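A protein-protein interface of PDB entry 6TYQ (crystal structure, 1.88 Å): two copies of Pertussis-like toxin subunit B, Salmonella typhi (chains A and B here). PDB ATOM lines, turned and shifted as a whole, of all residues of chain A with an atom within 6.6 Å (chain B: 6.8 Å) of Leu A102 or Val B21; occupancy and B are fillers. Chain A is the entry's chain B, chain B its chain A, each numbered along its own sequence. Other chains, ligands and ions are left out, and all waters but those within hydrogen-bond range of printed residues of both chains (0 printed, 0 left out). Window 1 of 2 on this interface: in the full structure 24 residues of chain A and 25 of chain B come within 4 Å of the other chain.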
ATOM      1  N   THR A   3     -27.714  34.974  11.620  1.00  0.00           N
ATOM      2  CA  THR A   3     -27.426  33.549  11.724  1.00  0.00           C
ATOM      3  C   THR A   3     -28.533  32.680  11.129  1.00  0.00           C
ATOM      4  O   THR A   3     -28.262  31.723  10.398  1.00  0.00           O
ATOM      5  CB  THR A   3     -27.211  33.189  13.202  1.00  0.00           C
ATOM      6  OG1 THR A   3     -26.089  33.920  13.703  1.00  0.00           O
ATOM      7  CG2 THR A   3     -26.950  31.700  13.352  1.00  0.00           C
ATOM      8  N   ILE A  16     -18.099  19.131  18.450  1.00  0.00           N
ATOM      9  CA  ILE A  16     -16.856  19.765  18.007  1.00  0.00           C
ATOM     10  C   ILE A  16     -15.698  18.838  18.351  1.00  0.00           C
ATOM     11  O   ILE A  16     -15.457  18.530  19.523  1.00  0.00           O
ATOM     12  CB  ILE A  16     -16.677  21.151  18.640  1.00  0.00           C
ATOM     13  CG1 ILE A  16     -17.846  22.068  18.239  1.00  0.00           C
ATOM     14  CG2 ILE A  16     -15.340  21.762  18.213  1.00  0.00           C
ATOM     15  CD1 ILE A  16     -17.766  23.511  18.762  1.00  0.00           C
ATOM     16  N   PHE A  30      -9.881  31.266  13.807  1.00  0.00           N
ATOM     17  CA  PHE A  30      -9.933  29.904  14.323  1.00  0.00           C
ATOM     18  C   PHE A  30     -10.799  29.056  13.399  1.00  0.00           C
ATOM     19  O   PHE A  30     -11.620  29.572  12.635  1.00  0.00           O
ATOM     20  CB  PHE A  30     -10.428  29.863  15.786  1.00  0.00           C
ATOM     21  CG  PHE A  30     -11.916  30.032  15.935  1.00  0.00           C
ATOM     22  CD1 PHE A  30     -12.472  31.299  16.000  1.00  0.00           C
ATOM     23  CD2 PHE A  30     -12.756  28.927  16.014  1.00  0.00           C
ATOM     24  CE1 PHE A  30     -13.845  31.461  16.142  1.00  0.00           C
ATOM     25  CE2 PHE A  30     -14.127  29.088  16.153  1.00  0.00           C
ATOM     26  CZ  PHE A  30     -14.667  30.365  16.220  1.00  0.00           C
ATOM     27  N   ILE A  32     -12.971  25.089  13.407  1.00  0.00           N
ATOM     28  CA  ILE A  32     -13.396  23.904  14.137  1.00  0.00           C
ATOM     29  C   ILE A  32     -13.789  22.822  13.146  1.00  0.00           C
ATOM     30  O   ILE A  32     -14.201  23.103  12.013  1.00  0.00           O
ATOM     31  CB  ILE A  32     -14.570  24.190  15.093  1.00  0.00           C
ATOM     32  CG1 ILE A  32     -15.700  24.883  14.348  1.00  0.00           C
ATOM     33  CG2 ILE A  32     -14.098  25.017  16.275  1.00  0.00           C
ATOM     34  CD1 ILE A  32     -16.965  25.005  15.181  1.00  0.00           C
ATOM     35  N   THR A  34     -16.308  19.351  13.152  1.00  0.00           N
ATOM     36  CA  THR A  34     -17.349  18.691  13.916  1.00  0.00           C
ATOM     37  C   THR A  34     -17.754  17.425  13.180  1.00  0.00           C
ATOM     38  O   THR A  34     -17.668  17.349  11.952  1.00  0.00           O
ATOM     39  CB  THR A  34     -18.576  19.593  14.133  1.00  0.00           C
ATOM     40  OG1 THR A  34     -19.356  19.640  12.933  1.00  0.00           O
ATOM     41  CG2 THR A  34     -18.149  21.018  14.514  1.00  0.00           C
ATOM     42  N   SER A  58     -18.743  39.193  15.514  1.00  0.00           N
ATOM     43  CA  SER A  58     -18.997  38.158  16.514  1.00  0.00           C
ATOM     44  C   SER A  58     -17.835  37.182  16.696  1.00  0.00           C
ATOM     45  O   SER A  58     -18.014  36.136  17.328  1.00  0.00           O
ATOM     46  CB  SER A  58     -20.271  37.391  16.169  1.00  0.00           C
ATOM     47  OG  SER A  58     -21.333  38.297  15.938  1.00  0.00           O
ATOM     48  N   GLU A  61     -17.107  36.203  20.407  1.00  0.00           N
ATOM     49  CA  GLU A  61     -18.163  35.418  21.044  1.00  0.00           C
ATOM     50  C   GLU A  61     -18.213  33.998  20.486  1.00  0.00           C
ATOM     51  O   GLU A  61     -18.474  33.043  21.221  1.00  0.00           O
ATOM     52  CB  GLU A  61     -19.496  36.125  20.859  1.00  0.00           C
ATOM     53  CG  GLU A  61     -19.637  37.388  21.711  1.00  0.00           C
ATOM     54  CD  GLU A  61     -18.974  38.643  21.122  1.00  0.00           C
ATOM     55  OE1 GLU A  61     -18.429  38.617  19.988  1.00  0.00           O
ATOM     56  OE2 GLU A  61     -19.015  39.681  21.810  1.00  0.00           O
ATOM     57  N   LEU A  62     -17.978  33.842  19.185  1.00  0.00           N
ATOM     58  CA  LEU A  62     -17.976  32.512  18.588  1.00  0.00           C
ATOM     59  C   LEU A  62     -16.767  31.700  19.029  1.00  0.00           C
ATOM     60  O   LEU A  62     -16.880  30.490  19.262  1.00  0.00           O
ATOM     61  CB  LEU A  62     -18.012  32.625  17.064  1.00  0.00           C
ATOM     62  CG  LEU A  62     -19.279  33.231  16.459  1.00  0.00           C
ATOM     63  CD1 LEU A  62     -19.012  33.600  15.005  1.00  0.00           C
ATOM     64  CD2 LEU A  62     -20.462  32.265  16.587  1.00  0.00           C
ATOM     65  N   LEU A  63     -15.596  32.334  19.124  1.00  0.00           N
ATOM     66  CA  LEU A  63     -14.416  31.623  19.615  1.00  0.00           C
ATOM     67  C   LEU A  63     -14.627  31.152  21.053  1.00  0.00           C
ATOM     68  O   LEU A  63     -14.350  29.995  21.395  1.00  0.00           O
ATOM     69  CB  LEU A  63     -13.174  32.522  19.513  1.00  0.00           C
ATOM     70  CG  LEU A  63     -11.840  31.922  19.986  1.00  0.00           C
ATOM     71  CD1 LEU A  63     -11.670  30.510  19.429  1.00  0.00           C
ATOM     72  CD2 LEU A  63     -10.672  32.808  19.575  1.00  0.00           C
ATOM     73  N   GLN A  65     -17.421  30.580  22.551  1.00  0.00           N
ATOM     74  CA  GLN A  65     -18.458  29.546  22.577  1.00  0.00           C
ATOM     75  C   GLN A  65     -17.964  28.238  21.967  1.00  0.00           C
ATOM     76  O   GLN A  65     -18.296  27.152  22.464  1.00  0.00           O
ATOM     77  CB  GLN A  65     -19.708  30.025  21.831  1.00  0.00           C
ATOM     78  CG  GLN A  65     -20.959  29.256  22.233  1.00  0.00           C
ATOM     79  CD  GLN A  65     -21.145  29.256  23.728  1.00  0.00           C
ATOM     80  OE1 GLN A  65     -21.122  30.312  24.360  1.00  0.00           O
ATOM     81  NE2 GLN A  65     -21.311  28.069  24.314  1.00  0.00           N
ATOM     82  N   ALA A  66     -17.199  28.314  20.875  1.00  0.00           N
ATOM     83  CA  ALA A  66     -16.613  27.099  20.310  1.00  0.00           C
ATOM     84  C   ALA A  66     -15.721  26.396  21.323  1.00  0.00           C
ATOM     85  O   ALA A  66     -15.791  25.169  21.480  1.00  0.00           O
ATOM     86  CB  ALA A  66     -15.826  27.424  19.040  1.00  0.00           C
ATOM     87  N   ARG A  67     -14.847  27.155  21.998  1.00  0.00           N
ATOM     88  CA  ARG A  67     -13.999  26.588  23.043  1.00  0.00           C
ATOM     89  C   ARG A  67     -14.824  25.892  24.111  1.00  0.00           C
ATOM     90  O   ARG A  67     -14.471  24.798  24.573  1.00  0.00           O
ATOM     91  CB  ARG A  67     -13.164  27.686  23.693  1.00  0.00           C
ATOM     92  CG  ARG A  67     -11.678  27.632  23.408  1.00  0.00           C
ATOM     93  CD  ARG A  67     -10.996  28.902  23.908  1.00  0.00           C
ATOM     94  NE  ARG A  67      -9.870  29.284  23.051  1.00  0.00           N
ATOM     95  CZ  ARG A  67      -9.504  30.540  22.831  1.00  0.00           C
ATOM     96  NH1 ARG A  67     -10.178  31.533  23.400  1.00  0.00           N
ATOM     97  NH2 ARG A  67      -8.462  30.807  22.056  1.00  0.00           N
ATOM     98  N   PHE A  69     -18.041  24.629  23.982  1.00  0.00           N
ATOM     99  CA  PHE A  69     -18.658  23.400  23.490  1.00  0.00           C
ATOM    100  C   PHE A  69     -17.614  22.332  23.175  1.00  0.00           C
ATOM    101  O   PHE A  69     -17.885  21.135  23.326  1.00  0.00           O
ATOM    102  CB  PHE A  69     -19.503  23.716  22.258  1.00  0.00           C
ATOM    103  CG  PHE A  69     -20.820  24.359  22.575  1.00  0.00           C
ATOM    104  CD1 PHE A  69     -21.466  24.104  23.782  1.00  0.00           C
ATOM    105  CD2 PHE A  69     -21.424  25.215  21.658  1.00  0.00           C
ATOM    106  CE1 PHE A  69     -22.707  24.696  24.066  1.00  0.00           C
ATOM    107  CE2 PHE A  69     -22.652  25.810  21.931  1.00  0.00           C
ATOM    108  CZ  PHE A  69     -23.298  25.543  23.135  1.00  0.00           C
ATOM    109  N   VAL A  76     -24.249  19.873  19.449  1.00  0.00           N
ATOM    110  CA  VAL A  76     -24.565  21.236  19.050  1.00  0.00           C
ATOM    111  C   VAL A  76     -25.046  21.258  17.607  1.00  0.00           C
ATOM    112  O   VAL A  76     -24.833  20.321  16.830  1.00  0.00           O
ATOM    113  CB  VAL A  76     -23.352  22.169  19.202  1.00  0.00           C
ATOM    114  CG1 VAL A  76     -22.847  22.159  20.640  1.00  0.00           C
ATOM    115  CG2 VAL A  76     -22.258  21.742  18.250  1.00  0.00           C
ATOM    116  N   ARG A  77     -25.709  22.347  17.258  1.00  0.00           N
ATOM    117  CA  ARG A  77     -25.999  22.664  15.870  1.00  0.00           C
ATOM    118  C   ARG A  77     -24.988  23.713  15.423  1.00  0.00           C
ATOM    119  O   ARG A  77     -24.817  24.730  16.101  1.00  0.00           O
ATOM    120  CB  ARG A  77     -27.432  23.179  15.696  1.00  0.00           C
ATOM    121  CG  ARG A  77     -27.747  23.614  14.262  1.00  0.00           C
ATOM    122  CD  ARG A  77     -29.208  24.039  14.073  1.00  0.00           C
ATOM    123  NE  ARG A  77     -30.111  22.902  14.256  1.00  0.00           N
ATOM    124  CZ  ARG A  77     -31.396  22.997  14.579  1.00  0.00           C
ATOM    125  NH1 ARG A  77     -31.954  24.188  14.761  1.00  0.00           N
ATOM    126  NH2 ARG A  77     -32.121  21.892  14.735  1.00  0.00           N
ATOM    127  N   ILE A  78     -24.303  23.441  14.304  1.00  0.00           N
ATOM    128  CA  ILE A  78     -23.345  24.365  13.686  1.00  0.00           C
ATOM    129  C   ILE A  78     -24.045  25.098  12.555  1.00  0.00           C
ATOM    130  O   ILE A  78     -24.596  24.461  11.653  1.00  0.00           O
ATOM    131  CB  ILE A  78     -22.112  23.628  13.127  1.00  0.00           C
ATOM    132  CG1 ILE A  78     -21.539  22.646  14.137  1.00  0.00           C
ATOM    133  CG2 ILE A  78     -21.038  24.634  12.659  1.00  0.00           C
ATOM    134  CD1 ILE A  78     -20.909  23.323  15.331  1.00  0.00           C
ATOM    135  N   HIS A  79     -23.988  26.429  12.580  1.00  0.00           N
ATOM    136  CA  HIS A  79     -24.532  27.286  11.535  1.00  0.00           C
ATOM    137  C   HIS A  79     -23.389  27.900  10.733  1.00  0.00           C
ATOM    138  O   HIS A  79     -22.460  28.467  11.312  1.00  0.00           O
ATOM    139  CB  HIS A  79     -25.394  28.398  12.140  1.00  0.00           C
ATOM    140  CG  HIS A  79     -26.404  27.910  13.137  1.00  0.00           C
ATOM    141  ND1 HIS A  79     -27.722  27.682  12.805  1.00  0.00           N
ATOM    142  CD2 HIS A  79     -26.290  27.618  14.457  1.00  0.00           C
ATOM    143  CE1 HIS A  79     -28.381  27.278  13.881  1.00  0.00           C
ATOM    144  NE2 HIS A  79     -27.534  27.223  14.895  1.00  0.00           N
ATOM    145  N   LEU A  99     -18.182  30.350   9.991  1.00  0.00           N
ATOM    146  CA  LEU A  99     -19.007  30.014  11.145  1.00  0.00           C
ATOM    147  C   LEU A  99     -19.880  31.207  11.512  1.00  0.00           C
ATOM    148  O   LEU A  99     -19.371  32.313  11.698  1.00  0.00           O
ATOM    149  CB  LEU A  99     -18.123  29.631  12.330  1.00  0.00           C
ATOM    150  CG  LEU A  99     -18.871  29.292  13.633  1.00  0.00           C
ATOM    151  CD1 LEU A  99     -19.636  27.989  13.433  1.00  0.00           C
ATOM    152  CD2 LEU A  99     -17.895  29.177  14.821  1.00  0.00           C
ATOM    153  N   VAL A 100     -21.192  30.999  11.646  1.00  0.00           N
ATOM    154  CA  VAL A 100     -22.089  32.112  11.945  1.00  0.00           C
ATOM    155  C   VAL A 100     -22.973  31.874  13.158  1.00  0.00           C
ATOM    156  O   VAL A 100     -23.739  32.768  13.525  1.00  0.00           O
ATOM    157  CB  VAL A 100     -22.958  32.504  10.728  1.00  0.00           C
ATOM    158  CG1 VAL A 100     -22.102  32.565   9.477  1.00  0.00           C
ATOM    159  CG2 VAL A 100     -24.120  31.536  10.535  1.00  0.00           C
ATOM    160  N   GLY A 101     -22.898  30.709  13.801  1.00  0.00           N
ATOM    161  CA  GLY A 101     -23.676  30.480  15.016  1.00  0.00           C
ATOM    162  C   GLY A 101     -23.420  29.095  15.579  1.00  0.00           C
ATOM    163  O   GLY A 101     -22.999  28.176  14.868  1.00  0.00           O
ATOM    164  N   LEU A 102     -23.671  28.967  16.886  1.00  0.00           N
ATOM    165  CA  LEU A 102     -23.572  27.687  17.581  1.00  0.00           C
ATOM    166  C   LEU A 102     -24.745  27.552  18.544  1.00  0.00           C
ATOM    167  O   LEU A 102     -25.048  28.497  19.270  1.00  0.00           O
ATOM    168  CB  LEU A 102     -22.257  27.578  18.353  1.00  0.00           C
ATOM    169  CG  LEU A 102     -21.008  27.481  17.475  1.00  0.00           C
ATOM    170  CD1 LEU A 102     -19.760  27.719  18.322  1.00  0.00           C
ATOM    171  CD2 LEU A 102     -20.976  26.110  16.822  1.00  0.00           C
ATOM    172  N   SER A 103     -25.401  26.393  18.548  1.00  0.00           N
ATOM    173  CA  SER A 103     -26.604  26.164  19.349  1.00  0.00           C
ATOM    174  C   SER A 103     -26.472  24.846  20.094  1.00  0.00           C
ATOM    175  O   SER A 103     -26.106  23.836  19.491  1.00  0.00           O
ATOM    176  CB  SER A 103     -27.886  26.128  18.480  1.00  0.00           C
ATOM    177  OG  SER A 103     -27.962  27.214  17.577  1.00  0.00           O
ATOM    178  N   SER A 104     -26.806  24.840  21.387  1.00  0.00           N
ATOM    179  CA  SER A 104     -26.878  23.576  22.111  1.00  0.00           C
ATOM    180  C   SER A 104     -28.085  22.758  21.641  1.00  0.00           C
ATOM    181  O   SER A 104     -29.084  23.299  21.171  1.00  0.00           O
ATOM    182  CB  SER A 104     -26.943  23.821  23.623  1.00  0.00           C
ATOM    183  OG  SER A 104     -28.116  24.522  23.985  1.00  0.00           O
ATOM    184  N   PHE A 111     -31.388  24.402  20.064  1.00  0.00           N
ATOM    185  CA  PHE A 111     -31.840  25.714  20.516  1.00  0.00           C
ATOM    186  C   PHE A 111     -31.285  26.784  19.580  1.00  0.00           C
ATOM    187  O   PHE A 111     -30.397  27.562  19.916  1.00  0.00           O
ATOM    188  CB  PHE A 111     -31.407  25.945  21.956  1.00  0.00           C
ATOM    189  CG  PHE A 111     -31.855  27.262  22.512  1.00  0.00           C
ATOM    190  CD1 PHE A 111     -33.207  27.578  22.536  1.00  0.00           C
ATOM    191  CD2 PHE A 111     -30.935  28.173  23.022  1.00  0.00           C
ATOM    192  CE1 PHE A 111     -33.653  28.794  23.046  1.00  0.00           C
ATOM    193  CE2 PHE A 111     -31.370  29.400  23.549  1.00  0.00           C
ATOM    194  CZ  PHE A 111     -32.736  29.709  23.556  1.00  0.00           C
ATOM    195  N   LEU B  19     -28.093  27.130  25.368  1.00  0.00           N
ATOM    196  CA  LEU B  19     -27.357  28.353  25.089  1.00  0.00           C
ATOM    197  C   LEU B  19     -27.072  28.418  23.597  1.00  0.00           C
ATOM    198  O   LEU B  19     -26.751  27.401  22.984  1.00  0.00           O
ATOM    199  CB  LEU B  19     -26.054  28.386  25.901  1.00  0.00           C
ATOM    200  CG  LEU B  19     -25.052  29.509  25.645  1.00  0.00           C
ATOM    201  CD1 LEU B  19     -25.656  30.862  25.936  1.00  0.00           C
ATOM    202  CD2 LEU B  19     -23.778  29.279  26.471  1.00  0.00           C
ATOM    203  N   HIS B  20     -27.201  29.614  23.020  1.00  0.00           N
ATOM    204  CA  HIS B  20     -27.009  29.846  21.596  1.00  0.00           C
ATOM    205  C   HIS B  20     -26.248  31.150  21.424  1.00  0.00           C
ATOM    206  O   HIS B  20     -26.490  32.112  22.157  1.00  0.00           O
ATOM    207  CB  HIS B  20     -28.360  29.918  20.862  1.00  0.00           C
ATOM    208  CG  HIS B  20     -28.285  30.537  19.497  1.00  0.00           C
ATOM    209  ND1 HIS B  20     -28.135  29.788  18.345  1.00  0.00           N
ATOM    210  CD2 HIS B  20     -28.364  31.829  19.097  1.00  0.00           C
ATOM    211  CE1 HIS B  20     -28.124  30.596  17.298  1.00  0.00           C
ATOM    212  NE2 HIS B  20     -28.250  31.841  17.728  1.00  0.00           N
ATOM    213  N   VAL B  21     -25.319  31.178  20.467  1.00  0.00           N
ATOM    214  CA  VAL B  21     -24.585  32.394  20.125  1.00  0.00           C
ATOM    215  C   VAL B  21     -24.705  32.621  18.624  1.00  0.00           C
ATOM    216  O   VAL B  21     -24.575  31.675  17.839  1.00  0.00           O
ATOM    217  CB  VAL B  21     -23.105  32.306  20.541  1.00  0.00           C
ATOM    218  CG1 VAL B  21     -22.328  33.450  19.931  1.00  0.00           C
ATOM    219  CG2 VAL B  21     -22.968  32.308  22.058  1.00  0.00           C
ATOM    220  N   GLY B  22     -24.968  33.870  18.225  1.00  0.00           N
ATOM    221  CA  GLY B  22     -25.171  34.191  16.824  1.00  0.00           C
ATOM    222  C   GLY B  22     -24.868  35.653  16.530  1.00  0.00           C
ATOM    223  O   GLY B  22     -24.302  36.354  17.377  1.00  0.00           O
ATOM    224  N   GLN B  23     -25.221  36.122  15.334  1.00  0.00           N
ATOM    225  CA  GLN B  23     -25.118  37.538  14.999  1.00  0.00           C
ATOM    226  C   GLN B  23     -26.377  37.967  14.258  1.00  0.00           C
ATOM    227  O   GLN B  23     -26.945  37.191  13.483  1.00  0.00           O
ATOM    228  CB  GLN B  23     -23.881  37.826  14.135  1.00  0.00           C
ATOM    229  CG  GLN B  23     -23.683  39.307  13.739  1.00  0.00           C
ATOM    230  CD  GLN B  23     -22.389  39.517  12.967  1.00  0.00           C
ATOM    231  OE1 GLN B  23     -21.311  39.116  13.420  1.00  0.00           O
ATOM    232  NE2 GLN B  23     -22.485  40.133  11.802  1.00  0.00           N
ATOM    233  N   PRO B  28     -23.242  40.825  17.643  1.00  0.00           N
ATOM    234  CA  PRO B  28     -23.239  39.531  18.336  1.00  0.00           C
ATOM    235  C   PRO B  28     -24.433  39.509  19.277  1.00  0.00           C
ATOM    236  O   PRO B  28     -24.830  40.543  19.816  1.00  0.00           O
ATOM    237  CB  PRO B  28     -21.911  39.523  19.109  1.00  0.00           C
ATOM    238  CG  PRO B  28     -21.074  40.639  18.495  1.00  0.00           C
ATOM    239  CD  PRO B  28     -22.039  41.630  17.930  1.00  0.00           C
ATOM    240  N   TYR B  29     -25.030  38.337  19.441  1.00  0.00           N
ATOM    241  CA  TYR B  29     -26.094  38.162  20.423  1.00  0.00           C
ATOM    242  C   TYR B  29     -25.977  36.768  21.009  1.00  0.00           C
ATOM    243  O   TYR B  29     -25.309  35.894  20.458  1.00  0.00           O
ATOM    244  CB  TYR B  29     -27.500  38.369  19.814  1.00  0.00           C
ATOM    245  CG  TYR B  29     -27.956  37.232  18.900  1.00  0.00           C
ATOM    246  CD1 TYR B  29     -27.658  37.242  17.541  1.00  0.00           C
ATOM    247  CD2 TYR B  29     -28.674  36.146  19.403  1.00  0.00           C
ATOM    248  CE1 TYR B  29     -28.068  36.205  16.706  1.00  0.00           C
ATOM    249  CE2 TYR B  29     -29.087  35.108  18.578  1.00  0.00           C
ATOM    250  CZ  TYR B  29     -28.775  35.140  17.234  1.00  0.00           C
ATOM    251  OH  TYR B  29     -29.173  34.099  16.421  1.00  0.00           O
ATOM    252  N   PHE B  30     -26.645  36.556  22.132  1.00  0.00           N
ATOM    253  CA  PHE B  30     -26.789  35.211  22.655  1.00  0.00           C
ATOM    254  C   PHE B  30     -28.181  35.069  23.233  1.00  0.00           C
ATOM    255  O   PHE B  30     -28.835  36.049  23.578  1.00  0.00           O
ATOM    256  CB  PHE B  30     -25.735  34.880  23.717  1.00  0.00           C
ATOM    257  CG  PHE B  30     -26.024  35.447  25.071  1.00  0.00           C
ATOM    258  CD1 PHE B  30     -25.606  36.727  25.395  1.00  0.00           C
ATOM    259  CD2 PHE B  30     -26.667  34.689  26.040  1.00  0.00           C
ATOM    260  CE1 PHE B  30     -25.844  37.265  26.660  1.00  0.00           C
ATOM    261  CE2 PHE B  30     -26.914  35.214  27.314  1.00  0.00           C
ATOM    262  CZ  PHE B  30     -26.493  36.508  27.624  1.00  0.00           C
ATOM    263  N   CYS B  31     -28.613  33.828  23.346  1.00  0.00           N
ATOM    264  CA  CYS B  31     -29.905  33.513  23.922  1.00  0.00           C
ATOM    265  C   CYS B  31     -29.731  32.364  24.895  1.00  0.00           C
ATOM    266  O   CYS B  31     -28.876  31.493  24.704  1.00  0.00           O
ATOM    267  CB  CYS B  31     -30.933  33.117  22.835  1.00  0.00           C
ATOM    268  SG  CYS B  31     -31.293  34.423  21.656  1.00  0.00           S
ATOM    269  N   LEU B  63     -23.518  37.750  29.267  1.00  0.00           N
ATOM    270  CA  LEU B  63     -23.026  36.573  28.551  1.00  0.00           C
ATOM    271  C   LEU B  63     -22.100  35.751  29.441  1.00  0.00           C
ATOM    272  O   LEU B  63     -22.259  34.531  29.555  1.00  0.00           O
ATOM    273  CB  LEU B  63     -22.325  36.991  27.245  1.00  0.00           C
ATOM    274  CG  LEU B  63     -21.650  35.874  26.436  1.00  0.00           C
ATOM    275  CD1 LEU B  63     -22.615  34.722  26.236  1.00  0.00           C
ATOM    276  CD2 LEU B  63     -21.166  36.391  25.076  1.00  0.00           C
ATOM    277  N   ARG B  67     -23.032  31.940  30.863  1.00  0.00           N
ATOM    278  CA  ARG B  67     -22.145  30.797  30.663  1.00  0.00           C
ATOM    279  C   ARG B  67     -21.742  30.181  31.992  1.00  0.00           C
ATOM    280  O   ARG B  67     -21.659  28.954  32.117  1.00  0.00           O
ATOM    281  CB  ARG B  67     -20.890  31.226  29.898  1.00  0.00           C
ATOM    282  CG  ARG B  67     -21.082  31.480  28.428  1.00  0.00           C
ATOM    283  CD  ARG B  67     -19.720  31.520  27.728  1.00  0.00           C
ATOM    284  NE  ARG B  67     -19.880  31.736  26.293  1.00  0.00           N
ATOM    285  CZ  ARG B  67     -19.352  32.753  25.636  1.00  0.00           C
ATOM    286  NH1 ARG B  67     -18.609  33.640  26.286  1.00  0.00           N
ATOM    287  NH2 ARG B  67     -19.557  32.876  24.331  1.00  0.00           N
ATOM    288  N   PHE B  94     -36.787  32.344  19.095  1.00  0.00           N
ATOM    289  CA  PHE B  94     -36.334  32.524  20.466  1.00  0.00           C
ATOM    290  C   PHE B  94     -37.481  33.156  21.238  1.00  0.00           C
ATOM    291  O   PHE B  94     -38.419  32.455  21.629  1.00  0.00           O
ATOM    292  CB  PHE B  94     -35.044  33.355  20.500  1.00  0.00           C
ATOM    293  CG  PHE B  94     -33.864  32.677  19.833  1.00  0.00           C
ATOM    294  CD1 PHE B  94     -33.353  31.498  20.330  1.00  0.00           C
ATOM    295  CD2 PHE B  94     -33.278  33.234  18.712  1.00  0.00           C
ATOM    296  CE1 PHE B  94     -32.256  30.879  19.727  1.00  0.00           C
ATOM    297  CE2 PHE B  94     -32.204  32.626  18.103  1.00  0.00           C
ATOM    298  CZ  PHE B  94     -31.688  31.445  18.611  1.00  0.00           C
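Of the 24 printed residues of chain A, 11 touch a printed residue of chain B. Printed residues of chain A that touch a printed residue of chain B: Thr A3, Ser A58, Glu A61, Gln A65, Phe A69, Val A100, Gly A101, Leu A102, Ser A103, Ser A104 and Phe A111. Hydrophobic or aromatic side chains of chain A within 4 Å of the printed part of chain B: Phe A69 and Phe A111. Along chain A the printed residues that touch a printed residue of chain B span positions 3 to 111.
Of chain B, only His B20 and Val B21 come within 4 Å of Leu A102. Printed residues of chain A within 4 Å of Leu B19: Gln A65 (3.5 Å), Phe A69 (3.9 Å), Ser A103 (3.8 Å), Ser A104 (3.0 Å) and Phe A111 (3.8 Å). Of the printed residues of chain B, Phe A69 touches Leu B19. Of the printed residues of chain A, His B20 touches Leu A102, Ser A103 and Phe A111. Of the printed residues of chain A, Phe B94 touches Phe A111. Of the printed residues of chain B, Glu A61 touches Pro B28 (3.6 Å), Leu B63 (3.8 Å) and Arg B67 (3.3 Å). Arg A67 touches none of the printed residues of chain B. Ile A78 touches none of the printed residues of chain B. The nearest residue of chain B that does not touch Leu A102 is Leu B19 (4.2 Å).
Among the printed residues, pairs that only touch across the chains: Thr A3 with Gly B22, Thr A3 with Tyr B29, Ser A58 with Gly B22, Ser A58 with Pro B28, Glu A61 with Pro B28, Glu A61 with Leu B63, Gln A65 with Leu B19, Gln A65 with Val B21, Phe A69 with Leu B19, Val A100 with Gly B22, Gly A101 with Val B21, Ser A103 with Leu B19, Phe A111 with Leu B19, Phe A111 with His B20, Phe A111 with Cys B31 and Phe A111 with Phe B94.
The backbone NH of Leu B19 is in hydrogen-bond range of the side-chain hydroxyl of Ser A104 (3.0 Å). A ring nitrogen (ND1) of His B20 sits close to the backbone carbonyl oxygen of Leu A102, 3.5 Å away. ND1 of His B20 is in hydrogen-bond range of OG of Ser A103 (2.7 Å). The backbone NH (N) of Val B21 is in hydrogen-bond range of the backbone carbonyl oxygen (O) of Leu A102. The backbone NH (N) of Gln B23 is in hydrogen-bond range of the side-chain hydroxyl (OG1) of Thr A3. The side-chain amide oxygen of Gln B23 lies within hydrogen-bond range of the side-chain hydroxyl of Ser A58 (2.6 Å). The guanidinium group (NH2) of Arg B67 lies within hydrogen-bond range of the backbone carbonyl oxygen (O) of Glu A61, 3.3 Å away. NE of Arg B67 is in hydrogen-bond range of OE1 of Gln A65.
Positions printed for both chains: 30, 63 and 67. Of the 24 pairs that touch across the chains among the printed residues, none has its exchanged pair printed and touching as well.
The backbone NH (N) of Cys B31 lies within hydrogen-bond range of the backbone carbonyl oxygen (O) of His B20. O of Gly B22 sits at hydrogen-bond distance from N of Tyr B29, at 3.0 Å. N of Arg A77 lies within hydrogen-bond range of O of Ser A103 (2.7 Å). The backbone carbonyl oxygen (O) of His A79 lies within hydrogen-bond range of the backbone NH (N) of Val A100, 2.9 Å away. The backbone NH of His A79 lies within hydrogen-bond range of the backbone carbonyl oxygen of Gly A101 (3.0 Å). O of Ser A104 is in hydrogen-bond range of N of Phe A111, 2.8 Å away.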
